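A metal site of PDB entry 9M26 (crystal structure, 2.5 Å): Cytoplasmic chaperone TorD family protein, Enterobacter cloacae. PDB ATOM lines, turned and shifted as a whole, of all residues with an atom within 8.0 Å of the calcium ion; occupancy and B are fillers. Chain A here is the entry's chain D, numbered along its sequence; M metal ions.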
ATOM      1  N   MET A   6       9.190 -26.476 -14.484  1.00  0.00           N
ATOM      2  CA  MET A   6      10.310 -25.723 -13.924  1.00  0.00           C
ATOM      3  C   MET A   6      10.367 -25.883 -12.410  1.00  0.00           C
ATOM      4  O   MET A   6      11.204 -25.271 -11.730  1.00  0.00           O
ATOM      5  CB  MET A   6      10.240 -24.231 -14.291  1.00  0.00           C
ATOM      6  CG  MET A   6       9.976 -23.930 -15.760  1.00  0.00           C
ATOM      7  SD  MET A   6      11.334 -24.344 -16.845  1.00  0.00           S
ATOM      8  CE  MET A   6      12.556 -23.098 -16.384  1.00  0.00           C
ATOM      9  N   PHE A   9      13.835 -26.790 -10.893  1.00  0.00           N
ATOM     10  CA  PHE A   9      14.935 -25.833 -10.927  1.00  0.00           C
ATOM     11  C   PHE A   9      14.930 -24.888  -9.722  1.00  0.00           C
ATOM     12  O   PHE A   9      15.863 -24.084  -9.572  1.00  0.00           O
ATOM     13  CB  PHE A   9      14.905 -25.030 -12.230  1.00  0.00           C
ATOM     14  CG  PHE A   9      15.135 -25.871 -13.463  1.00  0.00           C
ATOM     15  CD1 PHE A   9      14.098 -26.153 -14.332  1.00  0.00           C
ATOM     16  CD2 PHE A   9      16.386 -26.396 -13.745  1.00  0.00           C
ATOM     17  CE1 PHE A   9      14.298 -26.935 -15.470  1.00  0.00           C
ATOM     18  CE2 PHE A   9      16.586 -27.179 -14.873  1.00  0.00           C
ATOM     19  CZ  PHE A   9      15.543 -27.449 -15.731  1.00  0.00           C
ATOM     20  N   ASP A 181      15.777 -23.264 -22.083  1.00  0.00           N
ATOM     21  CA  ASP A 181      15.416 -24.349 -22.993  1.00  0.00           C
ATOM     22  C   ASP A 181      14.241 -25.160 -22.470  1.00  0.00           C
ATOM     23  O   ASP A 181      13.411 -25.648 -23.256  1.00  0.00           O
ATOM     24  CB  ASP A 181      16.633 -25.261 -23.226  1.00  0.00           C
ATOM     25  CG  ASP A 181      17.671 -24.602 -24.108  1.00  0.00           C
ATOM     26  OD1 ASP A 181      17.385 -23.502 -24.667  1.00  0.00           O
ATOM     27  OD2 ASP A 181      18.779 -25.182 -24.254  1.00  0.00           O
ATOM     28  N   GLU A 182      14.167 -25.373 -21.151  1.00  0.00           N
ATOM     29  CA  GLU A 182      13.064 -26.153 -20.601  1.00  0.00           C
ATOM     30  C   GLU A 182      11.762 -25.379 -20.629  1.00  0.00           C
ATOM     31  O   GLU A 182      10.709 -25.948 -20.935  1.00  0.00           O
ATOM     32  CB  GLU A 182      13.416 -26.613 -19.182  1.00  0.00           C
ATOM     33  CG  GLU A 182      12.458 -27.633 -18.567  1.00  0.00           C
ATOM     34  CD  GLU A 182      12.152 -28.828 -19.443  1.00  0.00           C
ATOM     35  OE1 GLU A 182      11.070 -29.420 -19.258  1.00  0.00           O
ATOM     36  OE2 GLU A 182      12.987 -29.224 -20.301  1.00  0.00           O
ATOM     37  N   LEU A 183      11.814 -24.068 -20.366  1.00  0.00           N
ATOM     38  CA  LEU A 183      10.587 -23.273 -20.437  1.00  0.00           C
ATOM     39  C   LEU A 183      10.000 -23.318 -21.842  1.00  0.00           C
ATOM     40  O   LEU A 183       8.811 -23.623 -22.012  1.00  0.00           O
ATOM     41  CB  LEU A 183      10.882 -21.837 -20.003  1.00  0.00           C
ATOM     42  N   GLU A 184      10.816 -23.051 -22.856  1.00  0.00           N
ATOM     43  CA  GLU A 184      10.330 -23.042 -24.224  1.00  0.00           C
ATOM     44  C   GLU A 184       9.804 -24.414 -24.634  1.00  0.00           C
ATOM     45  O   GLU A 184       8.787 -24.518 -25.318  1.00  0.00           O
ATOM     46  CB  GLU A 184      11.460 -22.595 -25.168  1.00  0.00           C
ATOM     47  N   GLU A 185      10.458 -25.481 -24.173  1.00  0.00           N
ATOM     48  CA  GLU A 185      10.085 -26.833 -24.550  1.00  0.00           C
ATOM     49  C   GLU A 185       8.761 -27.271 -23.927  1.00  0.00           C
ATOM     50  O   GLU A 185       8.038 -28.084 -24.529  1.00  0.00           O
ATOM     51  CB  GLU A 185      11.215 -27.785 -24.149  1.00  0.00           C
ATOM     52  CG  GLU A 185      10.959 -29.259 -24.266  1.00  0.00           C
ATOM     53  CD  GLU A 185      12.228 -30.060 -23.987  1.00  0.00           C
ATOM     54  OE1 GLU A 185      12.350 -30.635 -22.901  1.00  0.00           O
ATOM     55  OE2 GLU A 185      13.121 -30.066 -24.854  1.00  0.00           O
ATOM     56  N   GLU A 186       8.390 -26.732 -22.768  1.00  0.00           N
ATOM     57  CA  GLU A 186       7.106 -27.056 -22.183  1.00  0.00           C
ATOM     58  C   GLU A 186       5.991 -26.088 -22.574  1.00  0.00           C
ATOM     59  O   GLU A 186       4.816 -26.444 -22.447  1.00  0.00           O
ATOM     60  CB  GLU A 186       7.200 -27.123 -20.647  1.00  0.00           C
ATOM     61  CG  GLU A 186       8.181 -28.160 -20.071  1.00  0.00           C
ATOM     62  CD  GLU A 186       8.063 -29.549 -20.713  1.00  0.00           C
ATOM     63  OE1 GLU A 186       6.999 -30.175 -20.600  1.00  0.00           O
ATOM     64  OE2 GLU A 186       9.074 -30.052 -21.272  1.00  0.00           O
HETATM   65 CA    CA M   1      11.253 -31.197 -20.861  1.00  0.00          CA
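Three residues have an atom within 4 Å of the calcium ion: Glu 182, Glu 185 and Glu 186.
The side-chain carboxylate (OE1) of Glu 185 is bound to the calcium ion. OE1 of Glu 182 is bound to the calcium ion, at 2.4 Å. OE2 of Glu 186 is bound to the calcium ion. The calcium ion is bound by the side-chain carboxylate (OE2) of Glu 182, at 2.7 Å. The calcium ion has four donor atoms within binding distance.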
